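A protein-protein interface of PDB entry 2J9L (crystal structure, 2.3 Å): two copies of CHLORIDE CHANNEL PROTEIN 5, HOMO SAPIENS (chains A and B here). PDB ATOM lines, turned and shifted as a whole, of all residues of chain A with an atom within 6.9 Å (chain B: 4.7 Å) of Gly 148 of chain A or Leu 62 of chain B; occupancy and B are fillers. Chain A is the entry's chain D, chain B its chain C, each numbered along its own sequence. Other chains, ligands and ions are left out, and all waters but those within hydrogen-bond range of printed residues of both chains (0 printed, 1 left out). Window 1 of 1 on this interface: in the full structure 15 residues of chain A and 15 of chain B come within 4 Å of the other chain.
NH1 of Arg 61 of chain B lies within hydrogen-bond range of O of Asn 147 of chain A (3.1 Å). The guanidinium group (NH2) of Arg 149 of chain A lies close to the guanidinium group (NE) of Arg 61 of chain B, at 3.2 Å.
O of Ser 59 of chain A is in hydrogen-bond range of NE of Arg 149 of chain A (2.7 Å). The backbone carbonyl oxygen of Val 53 of chain B lies within hydrogen-bond range of the backbone NH of Val 63 of chain B (2.8 Å).
O of Leu 62 of chain A touches N of Gly 148 of chain B (3.8 Å). CA of Asn 147 of chain A touches O of Leu 62 of chain B, at 3.3 Å. CA of Val 63 of chain B touches OD1 of Asn 147 of chain A (3.7 Å). Gly 148 of chain A touches Leu 62 of chain B.
Gly 148 of chain A touches just one residue of chain B: Leu 62 (3.8 Å). Of chain A, only Asn 147 and Gly 148 come within 4 Å of Leu 62 of chain B. Printed residues of chain A within 4 Å of Gly 148 of chain B: Leu 62 (3.8 Å). Printed residues of chain B within 4 Å of Leu 62 of chain A: Gly 148. Printed residues of chain A within 4 Å of Arg 61 of chain B: Asn 147 and Arg 149. Of the printed residues of chain B, Arg 149 of chain A touches Arg 61. Of the printed residues of chain B, Asn 147 of chain A touches Arg 61, Leu 62 and Val 63. Val 54 of chain B touches none of the printed residues of chain A. The nearest residue of chain B that does not touch Gly 148 of chain A is Gly 148 of chain B (4.1 Å). The nearest residue of chain A that does not touch Leu 62 of chain B is His 146 of chain A (5.5 Å).
Of the 11 printed residues of chain A, 4 touch a printed residue of chain B.
Leu 62 of chain A touches Gly 148 of chain B, and with the chains exchanged Gly 148 of chain A touches Leu 62 of chain B. Positions printed for both chains: 60, 61, 62, 148 and 150.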
ATOM      1  N   SER A  59      23.340  22.187  37.102  1.00  0.00           N
ATOM      2  CA  SER A  59      22.019  22.101  36.502  1.00  0.00           C
ATOM      3  C   SER A  59      21.992  22.685  35.091  1.00  0.00           C
ATOM      4  O   SER A  59      21.256  22.201  34.231  1.00  0.00           O
ATOM      5  CB  SER A  59      20.987  22.817  37.369  1.00  0.00           C
ATOM      6  OG  SER A  59      21.079  24.218  37.199  1.00  0.00           O
ATOM      7  N   GLN A  60      22.800  23.719  34.865  1.00  0.00           N
ATOM      8  CA  GLN A  60      22.773  24.484  33.619  1.00  0.00           C
ATOM      9  C   GLN A  60      21.352  24.869  33.215  1.00  0.00           C
ATOM     10  O   GLN A  60      21.036  24.964  32.030  1.00  0.00           O
ATOM     11  CB  GLN A  60      23.488  23.740  32.483  1.00  0.00           C
ATOM     12  CG  GLN A  60      25.009  23.613  32.659  1.00  0.00           C
ATOM     13  CD  GLN A  60      25.755  24.947  32.570  1.00  0.00           C
ATOM     14  OE1 GLN A  60      25.281  25.910  31.961  1.00  0.00           O
ATOM     15  NE2 GLN A  60      26.939  24.998  33.172  1.00  0.00           N
ATOM     16  N   ARG A  61      20.492  25.088  34.200  1.00  0.00           N
ATOM     17  CA  ARG A  61      19.160  25.590  33.922  1.00  0.00           C
ATOM     18  C   ARG A  61      19.200  27.102  33.762  1.00  0.00           C
ATOM     19  O   ARG A  61      19.783  27.818  34.578  1.00  0.00           O
ATOM     20  CB  ARG A  61      18.166  25.156  35.000  1.00  0.00           C
ATOM     21  CG  ARG A  61      17.699  23.715  34.827  1.00  0.00           C
ATOM     22  CD  ARG A  61      16.627  23.326  35.828  1.00  0.00           C
ATOM     23  NE  ARG A  61      17.136  23.313  37.196  1.00  0.00           N
ATOM     24  CZ  ARG A  61      16.762  24.167  38.140  1.00  0.00           C
ATOM     25  NH1 ARG A  61      15.860  25.100  37.869  1.00  0.00           N
ATOM     26  NH2 ARG A  61      17.281  24.081  39.361  1.00  0.00           N
ATOM     27  N   LEU A  62      18.570  27.576  32.694  1.00  0.00           N
ATOM     28  CA  LEU A  62      18.739  28.936  32.233  1.00  0.00           C
ATOM     29  C   LEU A  62      17.897  29.890  33.049  1.00  0.00           C
ATOM     30  O   LEU A  62      16.718  29.637  33.287  1.00  0.00           O
ATOM     31  CB  LEU A  62      18.309  29.019  30.773  1.00  0.00           C
ATOM     32  CG  LEU A  62      19.139  29.785  29.747  1.00  0.00           C
ATOM     33  CD1 LEU A  62      18.256  30.068  28.545  1.00  0.00           C
ATOM     34  CD2 LEU A  62      19.699  31.062  30.305  1.00  0.00           C
ATOM     35  N   THR A 122      15.880  24.327  20.874  1.00  0.00           N
ATOM     36  CA  THR A 122      16.441  23.026  21.236  1.00  0.00           C
ATOM     37  C   THR A 122      17.588  22.695  20.299  1.00  0.00           C
ATOM     38  O   THR A 122      17.684  23.250  19.207  1.00  0.00           O
ATOM     39  CB  THR A 122      15.405  21.877  21.232  1.00  0.00           C
ATOM     40  OG1 THR A 122      14.931  21.644  19.903  1.00  0.00           O
ATOM     41  CG2 THR A 122      14.224  22.197  22.150  1.00  0.00           C
ATOM     42  N   THR A 145      19.263  24.721  23.877  1.00  0.00           N
ATOM     43  CA  THR A 145      19.037  23.836  25.008  1.00  0.00           C
ATOM     44  C   THR A 145      18.977  22.379  24.598  1.00  0.00           C
ATOM     45  O   THR A 145      18.624  22.055  23.469  1.00  0.00           O
ATOM     46  CB  THR A 145      17.729  24.176  25.744  1.00  0.00           C
ATOM     47  OG1 THR A 145      16.657  24.237  24.796  1.00  0.00           O
ATOM     48  CG2 THR A 145      17.844  25.510  26.456  1.00  0.00           C
ATOM     49  N   HIS A 146      19.344  21.506  25.530  1.00  0.00           N
ATOM     50  CA  HIS A 146      19.082  20.084  25.402  1.00  0.00           C
ATOM     51  C   HIS A 146      18.310  19.651  26.628  1.00  0.00           C
ATOM     52  O   HIS A 146      18.820  19.721  27.742  1.00  0.00           O
ATOM     53  CB  HIS A 146      20.371  19.275  25.293  1.00  0.00           C
ATOM     54  CG  HIS A 146      20.155  17.797  25.406  1.00  0.00           C
ATOM     55  ND1 HIS A 146      19.590  17.049  24.396  1.00  0.00           N
ATOM     56  CD2 HIS A 146      20.413  16.932  26.417  1.00  0.00           C
ATOM     57  CE1 HIS A 146      19.516  15.786  24.775  1.00  0.00           C
ATOM     58  NE2 HIS A 146      20.010  15.687  25.996  1.00  0.00           N
ATOM     59  N   ASN A 147      17.072  19.224  26.411  1.00  0.00           N
ATOM     60  CA  ASN A 147      16.198  18.780  27.488  1.00  0.00           C
ATOM     61  C   ASN A 147      16.114  19.754  28.643  1.00  0.00           C
ATOM     62  O   ASN A 147      16.197  19.361  29.802  1.00  0.00           O
ATOM     63  CB  ASN A 147      16.602  17.387  27.977  1.00  0.00           C
ATOM     64  CG  ASN A 147      16.145  16.298  27.036  1.00  0.00           C
ATOM     65  OD1 ASN A 147      15.482  16.574  26.040  1.00  0.00           O
ATOM     66  ND2 ASN A 147      16.499  15.057  27.339  1.00  0.00           N
ATOM     67  N   GLY A 148      15.950  21.030  28.317  1.00  0.00           N
ATOM     68  CA  GLY A 148      15.832  22.069  29.334  1.00  0.00           C
ATOM     69  C   GLY A 148      17.155  22.604  29.843  1.00  0.00           C
ATOM     70  O   GLY A 148      17.180  23.595  30.561  1.00  0.00           O
ATOM     71  N   ARG A 149      18.259  21.960  29.481  1.00  0.00           N
ATOM     72  CA  ARG A 149      19.569  22.392  29.966  1.00  0.00           C
ATOM     73  C   ARG A 149      20.317  23.225  28.927  1.00  0.00           C
ATOM     74  O   ARG A 149      20.248  22.949  27.731  1.00  0.00           O
ATOM     75  CB  ARG A 149      20.429  21.198  30.410  1.00  0.00           C
ATOM     76  CG  ARG A 149      19.653  20.037  31.021  1.00  0.00           C
ATOM     77  CD  ARG A 149      20.482  19.320  32.079  1.00  0.00           C
ATOM     78  NE  ARG A 149      20.237  19.898  33.394  1.00  0.00           N
ATOM     79  CZ  ARG A 149      19.808  19.216  34.449  1.00  0.00           C
ATOM     80  NH1 ARG A 149      19.604  19.844  35.599  1.00  0.00           N
ATOM     81  NH2 ARG A 149      19.603  17.909  34.364  1.00  0.00           N
ATOM     82  N   LEU A 150      21.029  24.246  29.394  1.00  0.00           N
ATOM     83  CA  LEU A 150      21.804  25.117  28.516  1.00  0.00           C
ATOM     84  C   LEU A 150      22.949  24.345  27.889  1.00  0.00           C
ATOM     85  O   LEU A 150      23.729  23.709  28.585  1.00  0.00           O
ATOM     86  CB  LEU A 150      22.341  26.317  29.295  1.00  0.00           C
ATOM     87  CG  LEU A 150      23.233  27.298  28.530  1.00  0.00           C
ATOM     88  CD1 LEU A 150      22.537  27.826  27.279  1.00  0.00           C
ATOM     89  CD2 LEU A 150      23.652  28.443  29.442  1.00  0.00           C
ATOM     90  N   PRO B  52       2.927  17.911  26.359  1.00  0.00           N
ATOM     91  CA  PRO B  52       4.371  17.994  26.521  1.00  0.00           C
ATOM     92  C   PRO B  52       4.887  16.652  26.993  1.00  0.00           C
ATOM     93  O   PRO B  52       4.208  15.970  27.749  1.00  0.00           O
ATOM     94  CB  PRO B  52       4.547  19.019  27.644  1.00  0.00           C
ATOM     95  CG  PRO B  52       3.255  19.748  27.731  1.00  0.00           C
ATOM     96  CD  PRO B  52       2.204  18.790  27.293  1.00  0.00           C
ATOM     97  N   VAL B  53       6.054  16.243  26.519  1.00  0.00           N
ATOM     98  CA  VAL B  53       6.727  15.136  27.172  1.00  0.00           C
ATOM     99  C   VAL B  53       7.978  15.630  27.882  1.00  0.00           C
ATOM    100  O   VAL B  53       8.734  16.463  27.367  1.00  0.00           O
ATOM    101  CB  VAL B  53       6.914  13.852  26.275  1.00  0.00           C
ATOM    102  CG1 VAL B  53       6.289  14.020  24.899  1.00  0.00           C
ATOM    103  CG2 VAL B  53       8.374  13.401  26.206  1.00  0.00           C
ATOM    104  N   VAL B  54       8.143  15.154  29.110  1.00  0.00           N
ATOM    105  CA  VAL B  54       9.197  15.631  29.989  1.00  0.00           C
ATOM    106  C   VAL B  54      10.139  14.498  30.335  1.00  0.00           C
ATOM    107  O   VAL B  54       9.775  13.336  30.245  1.00  0.00           O
ATOM    108  CB  VAL B  54       8.625  16.235  31.291  1.00  0.00           C
ATOM    109  CG1 VAL B  54       7.805  17.480  30.981  1.00  0.00           C
ATOM    110  CG2 VAL B  54       7.787  15.215  32.027  1.00  0.00           C
ATOM    111  N   GLN B  60      10.598  17.859  35.397  1.00  0.00           N
ATOM    112  CA  GLN B  60       9.762  18.653  34.493  1.00  0.00           C
ATOM    113  C   GLN B  60      10.603  19.312  33.399  1.00  0.00           C
ATOM    114  O   GLN B  60      10.321  20.426  32.967  1.00  0.00           O
ATOM    115  CB  GLN B  60       8.955  19.709  35.257  1.00  0.00           C
ATOM    116  CG  GLN B  60       7.925  19.145  36.226  1.00  0.00           C
ATOM    117  CD  GLN B  60       6.785  18.406  35.533  1.00  0.00           C
ATOM    118  OE1 GLN B  60       6.492  18.634  34.358  1.00  0.00           O
ATOM    119  NE2 GLN B  60       6.127  17.522  36.273  1.00  0.00           N
ATOM    120  N   ARG B  61      11.638  18.614  32.951  1.00  0.00           N
ATOM    121  CA  ARG B  61      12.460  19.117  31.864  1.00  0.00           C
ATOM    122  C   ARG B  61      11.889  18.713  30.498  1.00  0.00           C
ATOM    123  O   ARG B  61      11.708  17.532  30.212  1.00  0.00           O
ATOM    124  CB  ARG B  61      13.914  18.676  32.043  1.00  0.00           C
ATOM    125  CG  ARG B  61      14.602  19.398  33.196  1.00  0.00           C
ATOM    126  CD  ARG B  61      16.110  19.213  33.184  1.00  0.00           C
ATOM    127  NE  ARG B  61      16.512  17.907  33.698  1.00  0.00           N
ATOM    128  CZ  ARG B  61      17.027  16.937  32.953  1.00  0.00           C
ATOM    129  NH1 ARG B  61      17.210  17.125  31.654  1.00  0.00           N
ATOM    130  NH2 ARG B  61      17.370  15.783  33.511  1.00  0.00           N
ATOM    131  N   LEU B  62      11.604  19.715  29.672  1.00  0.00           N
ATOM    132  CA  LEU B  62      10.887  19.525  28.412  1.00  0.00           C
ATOM    133  C   LEU B  62      11.734  18.753  27.413  1.00  0.00           C
ATOM    134  O   LEU B  62      12.889  19.080  27.185  1.00  0.00           O
ATOM    135  CB  LEU B  62      10.517  20.882  27.825  1.00  0.00           C
ATOM    136  CG  LEU B  62       9.211  21.150  27.065  1.00  0.00           C
ATOM    137  CD1 LEU B  62       9.454  22.234  26.020  1.00  0.00           C
ATOM    138  CD2 LEU B  62       8.612  19.922  26.421  1.00  0.00           C
ATOM    139  N   VAL B  63      11.153  17.714  26.831  1.00  0.00           N
ATOM    140  CA  VAL B  63      11.812  16.955  25.782  1.00  0.00           C
ATOM    141  C   VAL B  63      11.160  17.305  24.453  1.00  0.00           C
ATOM    142  O   VAL B  63      11.829  17.425  23.436  1.00  0.00           O
ATOM    143  CB  VAL B  63      11.697  15.431  26.021  1.00  0.00           C
ATOM    144  CG1 VAL B  63      12.298  14.661  24.850  1.00  0.00           C
ATOM    145  CG2 VAL B  63      12.367  15.032  27.327  1.00  0.00           C
ATOM    146  N   GLY B  64       9.843  17.472  24.467  1.00  0.00           N
ATOM    147  CA  GLY B  64       9.111  17.747  23.235  1.00  0.00           C
ATOM    148  C   GLY B  64       7.613  17.841  23.435  1.00  0.00           C
ATOM    149  O   GLY B  64       7.132  17.845  24.562  1.00  0.00           O
ATOM    150  N   PRO B 118       9.805  22.087  20.299  1.00  0.00           N
ATOM    151  CA  PRO B 118       8.709  22.975  20.635  1.00  0.00           C
ATOM    152  C   PRO B 118       9.244  24.347  21.012  1.00  0.00           C
ATOM    153  O   PRO B 118      10.407  24.487  21.389  1.00  0.00           O
ATOM    154  CB  PRO B 118       8.079  22.304  21.852  1.00  0.00           C
ATOM    155  CG  PRO B 118       9.192  21.548  22.478  1.00  0.00           C
ATOM    156  CD  PRO B 118      10.037  21.067  21.335  1.00  0.00           C
ATOM    157  N   LEU B 143       5.019  26.466  25.001  1.00  0.00           N
ATOM    158  CA  LEU B 143       5.205  25.983  26.363  1.00  0.00           C
ATOM    159  C   LEU B 143       5.911  27.025  27.231  1.00  0.00           C
ATOM    160  O   LEU B 143       6.787  27.751  26.769  1.00  0.00           O
ATOM    161  CB  LEU B 143       5.957  24.649  26.369  1.00  0.00           C
ATOM    162  CG  LEU B 143       5.202  23.546  25.635  1.00  0.00           C
ATOM    163  CD1 LEU B 143       5.987  22.263  25.628  1.00  0.00           C
ATOM    164  CD2 LEU B 143       3.821  23.326  26.245  1.00  0.00           C
ATOM    165  N   GLY B 148      14.088  26.838  33.407  1.00  0.00           N
ATOM    166  CA  GLY B 148      14.367  25.592  32.706  1.00  0.00           C
ATOM    167  C   GLY B 148      13.405  24.468  33.017  1.00  0.00           C
ATOM    168  O   GLY B 148      13.618  23.339  32.590  1.00  0.00           O
ATOM    169  N   LEU B 150       9.407  23.060  32.853  1.00  0.00           N
ATOM    170  CA  LEU B 150       8.087  23.184  32.251  1.00  0.00           C
ATOM    171  C   LEU B 150       7.028  23.495  33.294  1.00  0.00           C
ATOM    172  O   LEU B 150       6.929  22.815  34.308  1.00  0.00           O
ATOM    173  CB  LEU B 150       7.722  21.898  31.507  1.00  0.00           C
ATOM    174  CG  LEU B 150       6.360  21.867  30.821  1.00  0.00           C
ATOM    175  CD1 LEU B 150       6.225  23.003  29.834  1.00  0.00           C
ATOM    176  CD2 LEU B 150       6.168  20.532  30.130  1.00  0.00           C
